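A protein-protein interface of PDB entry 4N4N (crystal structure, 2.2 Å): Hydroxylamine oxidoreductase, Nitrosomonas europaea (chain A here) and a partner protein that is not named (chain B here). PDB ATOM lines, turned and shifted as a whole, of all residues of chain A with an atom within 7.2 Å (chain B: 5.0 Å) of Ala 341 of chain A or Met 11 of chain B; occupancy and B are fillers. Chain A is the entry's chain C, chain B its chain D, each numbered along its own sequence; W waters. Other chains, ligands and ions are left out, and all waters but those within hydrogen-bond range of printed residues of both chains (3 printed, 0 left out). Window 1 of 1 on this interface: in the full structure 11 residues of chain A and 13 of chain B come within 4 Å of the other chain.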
ATOM      1  N   GLN A 196      -3.967  25.655  27.480  1.00  0.00           N
ATOM      2  CA  GLN A 196      -3.076  24.904  26.585  1.00  0.00           C
ATOM      3  C   GLN A 196      -3.087  23.408  26.909  1.00  0.00           C
ATOM      4  O   GLN A 196      -3.169  22.565  26.013  1.00  0.00           O
ATOM      5  CB  GLN A 196      -1.649  25.451  26.668  1.00  0.00           C
ATOM      6  CG  GLN A 196      -1.385  26.689  25.807  1.00  0.00           C
ATOM      7  CD  GLN A 196      -1.786  28.012  26.457  1.00  0.00           C
ATOM      8  OE1 GLN A 196      -2.388  28.050  27.534  1.00  0.00           O
ATOM      9  NE2 GLN A 196      -1.452  29.110  25.788  1.00  0.00           N
ATOM     10  N   ARG A 330       7.127  26.075  30.916  1.00  0.00           N
ATOM     11  CA  ARG A 330       6.711  26.985  29.840  1.00  0.00           C
ATOM     12  C   ARG A 330       6.400  26.241  28.538  1.00  0.00           C
ATOM     13  O   ARG A 330       5.363  26.473  27.916  1.00  0.00           O
ATOM     14  CB  ARG A 330       7.788  28.040  29.570  1.00  0.00           C
ATOM     15  CG  ARG A 330       8.113  28.980  30.735  1.00  0.00           C
ATOM     16  CD  ARG A 330       9.072  30.077  30.274  1.00  0.00           C
ATOM     17  NE  ARG A 330      10.147  29.488  29.491  1.00  0.00           N
ATOM     18  CZ  ARG A 330      10.720  30.029  28.422  1.00  0.00           C
ATOM     19  NH1 ARG A 330      10.364  31.225  27.962  1.00  0.00           N
ATOM     20  NH2 ARG A 330      11.671  29.353  27.817  1.00  0.00           N
ATOM     21  N   TRP A 331       7.309  25.356  28.130  1.00  0.00           N
ATOM     22  CA  TRP A 331       7.179  24.622  26.869  1.00  0.00           C
ATOM     23  C   TRP A 331       6.410  23.315  26.999  1.00  0.00           C
ATOM     24  O   TRP A 331       5.739  22.887  26.053  1.00  0.00           O
ATOM     25  CB  TRP A 331       8.554  24.340  26.276  1.00  0.00           C
ATOM     26  CG  TRP A 331       9.112  25.489  25.516  1.00  0.00           C
ATOM     27  CD1 TRP A 331      10.123  26.314  25.906  1.00  0.00           C
ATOM     28  CD2 TRP A 331       8.687  25.951  24.228  1.00  0.00           C
ATOM     29  NE1 TRP A 331      10.362  27.257  24.938  1.00  0.00           N
ATOM     30  CE2 TRP A 331       9.496  27.057  23.896  1.00  0.00           C
ATOM     31  CE3 TRP A 331       7.702  25.535  23.321  1.00  0.00           C
ATOM     32  CZ2 TRP A 331       9.347  27.763  22.698  1.00  0.00           C
ATOM     33  CZ3 TRP A 331       7.555  26.235  22.126  1.00  0.00           C
ATOM     34  CH2 TRP A 331       8.378  27.333  21.825  1.00  0.00           C
ATOM     35  N   TYR A 334       6.161  19.191  24.466  1.00  0.00           N
ATOM     36  CA  TYR A 334       5.629  19.121  23.098  1.00  0.00           C
ATOM     37  C   TYR A 334       5.346  20.528  22.546  1.00  0.00           C
ATOM     38  O   TYR A 334       4.316  21.128  22.865  1.00  0.00           O
ATOM     39  CB  TYR A 334       4.365  18.246  23.034  1.00  0.00           C
ATOM     40  CG  TYR A 334       4.515  16.848  23.620  1.00  0.00           C
ATOM     41  CD1 TYR A 334       4.999  15.790  22.847  1.00  0.00           C
ATOM     42  CD2 TYR A 334       4.156  16.583  24.944  1.00  0.00           C
ATOM     43  CE1 TYR A 334       5.134  14.504  23.382  1.00  0.00           C
ATOM     44  CE2 TYR A 334       4.284  15.301  25.489  1.00  0.00           C
ATOM     45  CZ  TYR A 334       4.773  14.269  24.702  1.00  0.00           C
ATOM     46  OH  TYR A 334       4.901  13.007  25.237  1.00  0.00           O
ATOM     47  N   PRO A 335       6.260  21.054  21.709  1.00  0.00           N
ATOM     48  CA  PRO A 335       6.210  22.454  21.270  1.00  0.00           C
ATOM     49  C   PRO A 335       5.080  22.749  20.281  1.00  0.00           C
ATOM     50  O   PRO A 335       4.770  23.916  20.035  1.00  0.00           O
ATOM     51  CB  PRO A 335       7.565  22.653  20.576  1.00  0.00           C
ATOM     52  CG  PRO A 335       8.390  21.448  20.935  1.00  0.00           C
ATOM     53  CD  PRO A 335       7.403  20.349  21.106  1.00  0.00           C
ATOM     54  N   PHE A 336       4.487  21.691  19.732  1.00  0.00           N
ATOM     55  CA  PHE A 336       3.424  21.796  18.731  1.00  0.00           C
ATOM     56  C   PHE A 336       2.023  21.916  19.333  1.00  0.00           C
ATOM     57  O   PHE A 336       1.059  22.144  18.602  1.00  0.00           O
ATOM     58  CB  PHE A 336       3.479  20.594  17.774  1.00  0.00           C
ATOM     59  CG  PHE A 336       3.336  19.261  18.461  1.00  0.00           C
ATOM     60  CD1 PHE A 336       2.080  18.678  18.627  1.00  0.00           C
ATOM     61  CD2 PHE A 336       4.458  18.591  18.949  1.00  0.00           C
ATOM     62  CE1 PHE A 336       1.940  17.446  19.270  1.00  0.00           C
ATOM     63  CE2 PHE A 336       4.335  17.363  19.586  1.00  0.00           C
ATOM     64  CZ  PHE A 336       3.071  16.785  19.752  1.00  0.00           C
ATOM     65  N   VAL A 337       1.901  21.748  20.651  1.00  0.00           N
ATOM     66  CA  VAL A 337       0.596  21.868  21.315  1.00  0.00           C
ATOM     67  C   VAL A 337       0.039  23.279  21.090  1.00  0.00           C
ATOM     68  O   VAL A 337       0.721  24.266  21.388  1.00  0.00           O
ATOM     69  CB  VAL A 337       0.666  21.515  22.828  1.00  0.00           C
ATOM     70  CG1 VAL A 337      -0.596  21.978  23.573  1.00  0.00           C
ATOM     71  CG2 VAL A 337       0.865  20.020  23.022  1.00  0.00           C
ATOM     72  N   PRO A 338      -1.187  23.378  20.528  1.00  0.00           N
ATOM     73  CA  PRO A 338      -1.773  24.688  20.220  1.00  0.00           C
ATOM     74  C   PRO A 338      -1.758  25.641  21.413  1.00  0.00           C
ATOM     75  O   PRO A 338      -2.087  25.250  22.539  1.00  0.00           O
ATOM     76  CB  PRO A 338      -3.207  24.342  19.811  1.00  0.00           C
ATOM     77  CG  PRO A 338      -3.082  22.967  19.217  1.00  0.00           C
ATOM     78  CD  PRO A 338      -2.060  22.272  20.086  1.00  0.00           C
ATOM     79  N   GLY A 339      -1.342  26.875  21.154  1.00  0.00           N
ATOM     80  CA  GLY A 339      -1.271  27.898  22.182  1.00  0.00           C
ATOM     81  C   GLY A 339       0.059  27.991  22.905  1.00  0.00           C
ATOM     82  O   GLY A 339       0.310  28.983  23.590  1.00  0.00           O
ATOM     83  N   ILE A 340       0.908  26.970  22.764  1.00  0.00           N
ATOM     84  CA  ILE A 340       2.190  26.920  23.489  1.00  0.00           C
ATOM     85  C   ILE A 340       3.239  27.887  22.936  1.00  0.00           C
ATOM     86  O   ILE A 340       3.832  28.661  23.690  1.00  0.00           O
ATOM     87  CB  ILE A 340       2.763  25.470  23.598  1.00  0.00           C
ATOM     88  CG1 ILE A 340       1.853  24.584  24.466  1.00  0.00           C
ATOM     89  CG2 ILE A 340       4.199  25.473  24.143  1.00  0.00           C
ATOM     90  CD1 ILE A 340       1.819  24.944  25.955  1.00  0.00           C
ATOM     91  N   ALA A 341       3.476  27.828  21.628  1.00  0.00           N
ATOM     92  CA  ALA A 341       4.431  28.725  20.977  1.00  0.00           C
ATOM     93  C   ALA A 341       3.996  30.190  21.095  1.00  0.00           C
ATOM     94  O   ALA A 341       4.808  31.065  21.402  1.00  0.00           O
ATOM     95  CB  ALA A 341       4.616  28.338  19.523  1.00  0.00           C
ATOM     96  N   GLU A 342       2.706  30.438  20.865  1.00  0.00           N
ATOM     97  CA  GLU A 342       2.129  31.785  20.946  1.00  0.00           C
ATOM     98  C   GLU A 342       2.238  32.378  22.360  1.00  0.00           C
ATOM     99  O   GLU A 342       2.321  33.595  22.526  1.00  0.00           O
ATOM    100  CB  GLU A 342       0.662  31.771  20.490  1.00  0.00           C
ATOM    101  CG  GLU A 342       0.436  31.367  19.023  1.00  0.00           C
ATOM    102  CD  GLU A 342       0.308  29.858  18.804  1.00  0.00           C
ATOM    103  OE1 GLU A 342       0.559  29.071  19.740  1.00  0.00           O
ATOM    104  OE2 GLU A 342      -0.051  29.452  17.681  1.00  0.00           O
ATOM    105  N   ASN A 343       2.254  31.501  23.364  1.00  0.00           N
ATOM    106  CA  ASN A 343       2.304  31.892  24.769  1.00  0.00           C
ATOM    107  C   ASN A 343       3.720  32.178  25.290  1.00  0.00           C
ATOM    108  O   ASN A 343       3.882  32.701  26.395  1.00  0.00           O
ATOM    109  CB  ASN A 343       1.616  30.815  25.627  1.00  0.00           C
ATOM    110  CG  ASN A 343       1.623  31.140  27.112  1.00  0.00           C
ATOM    111  OD1 ASN A 343       1.136  32.194  27.536  1.00  0.00           O
ATOM    112  ND2 ASN A 343       2.182  30.233  27.912  1.00  0.00           N
ATOM    113  N   ILE A 344       4.739  31.854  24.492  1.00  0.00           N
ATOM    114  CA  ILE A 344       6.136  31.972  24.942  1.00  0.00           C
ATOM    115  C   ILE A 344       6.597  33.413  25.226  1.00  0.00           C
ATOM    116  O   ILE A 344       7.571  33.623  25.952  1.00  0.00           O
ATOM    117  CB  ILE A 344       7.128  31.215  24.002  1.00  0.00           C
ATOM    118  CG1 ILE A 344       8.307  30.650  24.804  1.00  0.00           C
ATOM    119  CG2 ILE A 344       7.608  32.097  22.841  1.00  0.00           C
ATOM    120  CD1 ILE A 344       7.924  29.537  25.766  1.00  0.00           C
ATOM    121  N   THR A 345       5.887  34.392  24.663  1.00  0.00           N
ATOM    122  CA  THR A 345       6.217  35.809  24.845  1.00  0.00           C
ATOM    123  C   THR A 345       5.435  36.475  25.986  1.00  0.00           C
ATOM    124  O   THR A 345       5.759  37.592  26.393  1.00  0.00           O
ATOM    125  CB  THR A 345       5.975  36.612  23.547  1.00  0.00           C
ATOM    126  OG1 THR A 345       4.628  36.411  23.102  1.00  0.00           O
ATOM    127  CG2 THR A 345       6.935  36.172  22.448  1.00  0.00           C
ATOM    128  N   SER A 346       4.418  35.788  26.501  1.00  0.00           N
ATOM    129  CA  SER A 346       3.523  36.355  27.514  1.00  0.00           C
ATOM    130  C   SER A 346       4.227  36.649  28.842  1.00  0.00           C
ATOM    131  O   SER A 346       5.292  36.092  29.130  1.00  0.00           O
ATOM    132  CB  SER A 346       2.315  35.436  27.740  1.00  0.00           C
ATOM    133  OG  SER A 346       2.648  34.335  28.570  1.00  0.00           O
ATOM    134  N   LYS A 378      14.361  29.894  20.798  1.00  0.00           N
ATOM    135  CA  LYS A 378      14.417  30.117  19.353  1.00  0.00           C
ATOM    136  C   LYS A 378      14.707  28.837  18.577  1.00  0.00           C
ATOM    137  O   LYS A 378      14.119  28.601  17.520  1.00  0.00           O
ATOM    138  CB  LYS A 378      15.428  31.216  19.008  1.00  0.00           C
ATOM    139  CG  LYS A 378      14.922  32.615  19.324  1.00  0.00           C
ATOM    140  CD  LYS A 378      15.956  33.683  19.011  1.00  0.00           C
ATOM    141  CE  LYS A 378      15.528  35.028  19.571  1.00  0.00           C
ATOM    142  NZ  LYS A 378      16.696  35.943  19.730  1.00  0.00           N
ATOM    143  N   LEU A 381      11.482  26.824  18.358  1.00  0.00           N
ATOM    144  CA  LEU A 381      10.572  27.372  17.356  1.00  0.00           C
ATOM    145  C   LEU A 381      11.024  27.051  15.935  1.00  0.00           C
ATOM    146  O   LEU A 381      10.195  26.800  15.060  1.00  0.00           O
ATOM    147  CB  LEU A 381      10.424  28.886  17.534  1.00  0.00           C
ATOM    148  CG  LEU A 381       9.570  29.373  18.701  1.00  0.00           C
ATOM    149  CD1 LEU A 381       9.799  30.862  18.949  1.00  0.00           C
ATOM    150  CD2 LEU A 381       8.093  29.079  18.455  1.00  0.00           C
ATOM    151  N   LEU A 384       9.908  23.681  15.252  1.00  0.00           N
ATOM    152  CA  LEU A 384       8.462  23.726  15.037  1.00  0.00           C
ATOM    153  C   LEU A 384       8.099  24.215  13.633  1.00  0.00           C
ATOM    154  O   LEU A 384       7.214  23.652  12.990  1.00  0.00           O
ATOM    155  CB  LEU A 384       7.784  24.591  16.110  1.00  0.00           C
ATOM    156  CG  LEU A 384       6.264  24.798  16.075  1.00  0.00           C
ATOM    157  CD1 LEU A 384       5.487  23.485  16.192  1.00  0.00           C
ATOM    158  CD2 LEU A 384       5.863  25.759  17.176  1.00  0.00           C
ATOM    159  N   GLN A 388       5.912  22.302  10.854  1.00  0.00           N
ATOM    160  CA  GLN A 388       4.712  22.968  10.344  1.00  0.00           C
ATOM    161  C   GLN A 388       4.671  23.009   8.816  1.00  0.00           C
ATOM    162  O   GLN A 388       3.612  22.814   8.220  1.00  0.00           O
ATOM    163  CB  GLN A 388       4.561  24.373  10.938  1.00  0.00           C
ATOM    164  CG  GLN A 388       4.100  24.385  12.411  1.00  0.00           C
ATOM    165  CD  GLN A 388       4.066  25.781  13.007  1.00  0.00           C
ATOM    166  OE1 GLN A 388       4.706  26.709  12.502  1.00  0.00           O
ATOM    167  NE2 GLN A 388       3.312  25.939  14.087  1.00  0.00           N
ATOM    168  N   ILE B   6      -0.379  31.627  15.726  1.00  0.00           N
ATOM    169  CA  ILE B   6       0.710  32.307  15.031  1.00  0.00           C
ATOM    170  C   ILE B   6       1.788  31.278  14.703  1.00  0.00           C
ATOM    171  O   ILE B   6       2.283  30.580  15.597  1.00  0.00           O
ATOM    172  CB  ILE B   6       1.326  33.465  15.866  1.00  0.00           C
ATOM    173  CG1 ILE B   6       0.240  34.425  16.368  1.00  0.00           C
ATOM    174  CG2 ILE B   6       2.368  34.223  15.045  1.00  0.00           C
ATOM    175  CD1 ILE B   6       0.712  35.408  17.434  1.00  0.00           C
ATOM    176  N   SER B   7       2.144  31.185  13.425  1.00  0.00           N
ATOM    177  CA  SER B   7       3.135  30.211  12.968  1.00  0.00           C
ATOM    178  C   SER B   7       4.493  30.461  13.618  1.00  0.00           C
ATOM    179  O   SER B   7       4.819  31.598  13.979  1.00  0.00           O
ATOM    180  CB  SER B   7       3.255  30.221  11.440  1.00  0.00           C
ATOM    181  OG  SER B   7       4.036  31.310  10.988  1.00  0.00           O
ATOM    182  N   ALA B   8       5.272  29.392  13.768  1.00  0.00           N
ATOM    183  CA  ALA B   8       6.587  29.464  14.402  1.00  0.00           C
ATOM    184  C   ALA B   8       7.520  30.453  13.703  1.00  0.00           C
ATOM    185  O   ALA B   8       8.245  31.199  14.363  1.00  0.00           O
ATOM    186  CB  ALA B   8       7.220  28.087  14.477  1.00  0.00           C
ATOM    187  N   LYS B   9       7.481  30.468  12.372  1.00  0.00           N
ATOM    188  CA  LYS B   9       8.302  31.389  11.585  1.00  0.00           C
ATOM    189  C   LYS B   9       7.966  32.852  11.892  1.00  0.00           C
ATOM    190  O   LYS B   9       8.868  33.689  11.990  1.00  0.00           O
ATOM    191  CB  LYS B   9       8.205  31.079  10.082  1.00  0.00           C
ATOM    192  CG  LYS B   9       7.177  31.876   9.295  1.00  0.00           C
ATOM    193  CD  LYS B   9       7.143  31.448   7.829  1.00  0.00           C
ATOM    194  CE  LYS B   9       6.681  32.589   6.919  1.00  0.00           C
ATOM    195  NZ  LYS B   9       5.382  33.189   7.337  1.00  0.00           N
ATOM    196  N   ASP B  10       6.675  33.141  12.069  1.00  0.00           N
ATOM    197  CA  ASP B  10       6.224  34.483  12.424  1.00  0.00           C
ATOM    198  C   ASP B  10       6.592  34.827  13.868  1.00  0.00           C
ATOM    199  O   ASP B  10       6.952  35.966  14.164  1.00  0.00           O
ATOM    200  CB  ASP B  10       4.715  34.649  12.177  1.00  0.00           C
ATOM    201  CG  ASP B  10       4.357  34.643  10.693  1.00  0.00           C
ATOM    202  OD1 ASP B  10       3.262  34.166  10.338  1.00  0.00           O
ATOM    203  OD2 ASP B  10       5.174  35.108   9.873  1.00  0.00           O
ATOM    204  N   MET B  11       6.518  33.834  14.751  1.00  0.00           N
ATOM    205  CA  MET B  11       6.967  33.981  16.139  1.00  0.00           C
ATOM    206  C   MET B  11       8.459  34.307  16.218  1.00  0.00           C
ATOM    207  O   MET B  11       8.877  35.125  17.031  1.00  0.00           O
ATOM    208  CB  MET B  11       6.660  32.718  16.950  1.00  0.00           C
ATOM    209  CG  MET B  11       5.187  32.520  17.313  1.00  0.00           C
ATOM    210  SD  MET B  11       4.438  33.883  18.237  1.00  0.00           S
ATOM    211  CE  MET B  11       5.485  33.976  19.692  1.00  0.00           C
ATOM    212  N   LEU B  12       9.248  33.663  15.361  1.00  0.00           N
ATOM    213  CA  LEU B  12      10.696  33.874  15.282  1.00  0.00           C
ATOM    214  C   LEU B  12      11.049  35.268  14.763  1.00  0.00           C
ATOM    215  O   LEU B  12      11.921  35.939  15.315  1.00  0.00           O
ATOM    216  CB  LEU B  12      11.327  32.811  14.382  1.00  0.00           C
ATOM    217  CG  LEU B  12      12.212  31.663  14.893  1.00  0.00           C
ATOM    218  CD1 LEU B  12      12.384  31.579  16.415  1.00  0.00           C
ATOM    219  CD2 LEU B  12      11.742  30.336  14.298  1.00  0.00           C
ATOM    220  N   ASP B  13      10.372  35.687  13.697  1.00  0.00           N
ATOM    221  CA  ASP B  13      10.572  37.014  13.122  1.00  0.00           C
ATOM    222  C   ASP B  13      10.191  38.097  14.126  1.00  0.00           C
ATOM    223  O   ASP B  13      10.899  39.098  14.264  1.00  0.00           O
ATOM    224  CB  ASP B  13       9.776  37.167  11.821  1.00  0.00           C
ATOM    225  CG  ASP B  13      10.283  36.262  10.709  1.00  0.00           C
ATOM    226  OD1 ASP B  13      11.394  35.702  10.843  1.00  0.00           O
ATOM    227  OD2 ASP B  13       9.568  36.114   9.694  1.00  0.00           O
ATOM    228  N   TYR B  14       9.087  37.875  14.837  1.00  0.00           N
ATOM    229  CA  TYR B  14       8.647  38.771  15.904  1.00  0.00           C
ATOM    230  C   TYR B  14       9.691  38.905  17.014  1.00  0.00           C
ATOM    231  O   TYR B  14       9.942  40.010  17.499  1.00  0.00           O
ATOM    232  CB  TYR B  14       7.305  38.305  16.483  1.00  0.00           C
ATOM    233  CG  TYR B  14       6.748  39.209  17.561  1.00  0.00           C
ATOM    234  CD1 TYR B  14       6.176  40.438  17.239  1.00  0.00           C
ATOM    235  CD2 TYR B  14       6.793  38.832  18.905  1.00  0.00           C
ATOM    236  CE1 TYR B  14       5.664  41.272  18.222  1.00  0.00           C
ATOM    237  CE2 TYR B  14       6.279  39.662  19.902  1.00  0.00           C
ATOM    238  CZ  TYR B  14       5.718  40.879  19.550  1.00  0.00           C
ATOM    239  OH  TYR B  14       5.206  41.708  20.519  1.00  0.00           O
ATOM    240  N   LEU B  15      10.288  37.780  17.410  1.00  0.00           N
ATOM    241  CA  LEU B  15      11.321  37.772  18.446  1.00  0.00           C
ATOM    242  C   LEU B  15      12.625  38.402  17.962  1.00  0.00           C
ATOM    243  O   LEU B  15      13.296  39.101  18.721  1.00  0.00           O
ATOM    244  CB  LEU B  15      11.571  36.354  18.964  1.00  0.00           C
ATOM    245  CG  LEU B  15      10.564  35.787  19.968  1.00  0.00           C
ATOM    246  CD1 LEU B  15      10.740  34.281  20.085  1.00  0.00           C
ATOM    247  CD2 LEU B  15      10.690  36.458  21.337  1.00  0.00           C
ATOM    248  N   ARG B  53      -3.007  39.228  18.139  1.00  0.00           N
ATOM    249  CA  ARG B  53      -3.225  39.500  19.560  1.00  0.00           C
ATOM    250  C   ARG B  53      -4.575  40.188  19.789  1.00  0.00           C
ATOM    251  O   ARG B  53      -5.157  40.089  20.872  1.00  0.00           O
ATOM    252  CB  ARG B  53      -2.085  40.352  20.136  1.00  0.00           C
ATOM    253  CG  ARG B  53      -0.715  39.667  20.158  1.00  0.00           C
ATOM    254  CD  ARG B  53      -0.530  38.767  21.381  1.00  0.00           C
ATOM    255  NE  ARG B  53       0.809  38.180  21.433  1.00  0.00           N
ATOM    256  CZ  ARG B  53       1.099  36.914  21.137  1.00  0.00           C
ATOM    257  NH1 ARG B  53       0.145  36.065  20.769  1.00  0.00           N
ATOM    258  NH2 ARG B  53       2.354  36.490  21.216  1.00  0.00           N
HETATM  259  O   HOH W   1      15.400  38.341  19.979  1.00  0.00           O
HETATM  260  O   HOH W   2       3.182  27.923  16.140  1.00  0.00           O
HETATM  261  O   HOH W   3       6.044  28.220  10.875  1.00  0.00           O
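Among the printed residues, merely in contact across the chains: Leu 381 of chain A with Ala 8 of chain B, Ala 341 of chain A with Met 11 of chain B, Leu 381 of chain A with Leu 12 of chain B, Lys 378 of chain A with Leu 12 of chain B, Leu 381 of chain A with Leu 15 of chain B, Leu 384 of chain A with Ala 8 of chain B, Thr 345 of chain A with Met 11 of chain B, Gln 388 of chain A with Ser 7 of chain B and Thr 345 of chain A with Leu 15 of chain B.
OE2 of Glu 342 of chain A is in hydrogen-bond range of N of Ile 6 of chain B (2.9 Å).
The backbone carbonyl oxygen of Glu 342 of chain A lies within hydrogen-bond range of the guanidinium group of Arg 53 of chain B, 3.2 Å away.
The side-chain hydroxyl of Thr 345 of chain A sits at hydrogen-bond distance from the guanidinium group of Arg 53 of chain B (3.0 Å).
The backbone NH (N) of Ala 8 of chain B lies within hydrogen-bond range of the side-chain amide oxygen (OE1) of Gln 388 of chain A (3.0 Å).
Of the 20 printed residues of chain A, 7 touch a printed residue of chain B.
Hydrophobic or aromatic side chains of chain A within 4 Å of the printed part of chain B: Leu 381 and Leu 384.
Along chain B the printed residues that touch a printed residue of chain A span positions 6 to 53.
Among the printed residues, no Asp or Glu carboxylate lies within 4 Å of a Lys or Arg side-chain nitrogen of the other chain.
The backbone NH (N) of Gly 339 of chain A sits at hydrogen-bond distance from the side-chain carboxylate (OE1) of Glu 342 of chain A (3.2 Å).
OG of Ser 7 of chain B lies within hydrogen-bond range of OD1 of Asp 10 of chain B, at 3.0 Å.
Of the printed residues of chain B, Ala 341 of chain A touches Met 11 (3.4 Å).
Met 11 of chain B touches two residues of chain A.
Printed residues of chain A within 4 Å of Leu 15 of chain B: Thr 345 and Leu 381.
Of the printed residues of chain A, Arg 53 of chain B touches Glu 342 (3.2 Å) and Thr 345 (3.0 Å).
The nearest printed residue of chain A that does not touch Ile 6 of chain B is Gln 388 of chain A (5.0 Å).
Water W1 lies within hydrogen-bond range of O of Leu 15 of chain B (2.6 Å) and NZ of Lys 378 of chain A (2.7 Å).
Water W3 lies within hydrogen-bond range of the side-chain amide oxygen of Gln 388 of chain A, the backbone NH of Lys 9 of chain B and the backbone NH of Ala 8 of chain B.
Water W2 lies within hydrogen-bond range of the backbone carbonyl oxygen (O) of Ile 6 of chain B (2.9 Å), the side-chain amide nitrogen (NE2) of Gln 388 of chain A (2.9 Å) and the backbone NH (N) of Ala 8 of chain B (3.5 Å).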
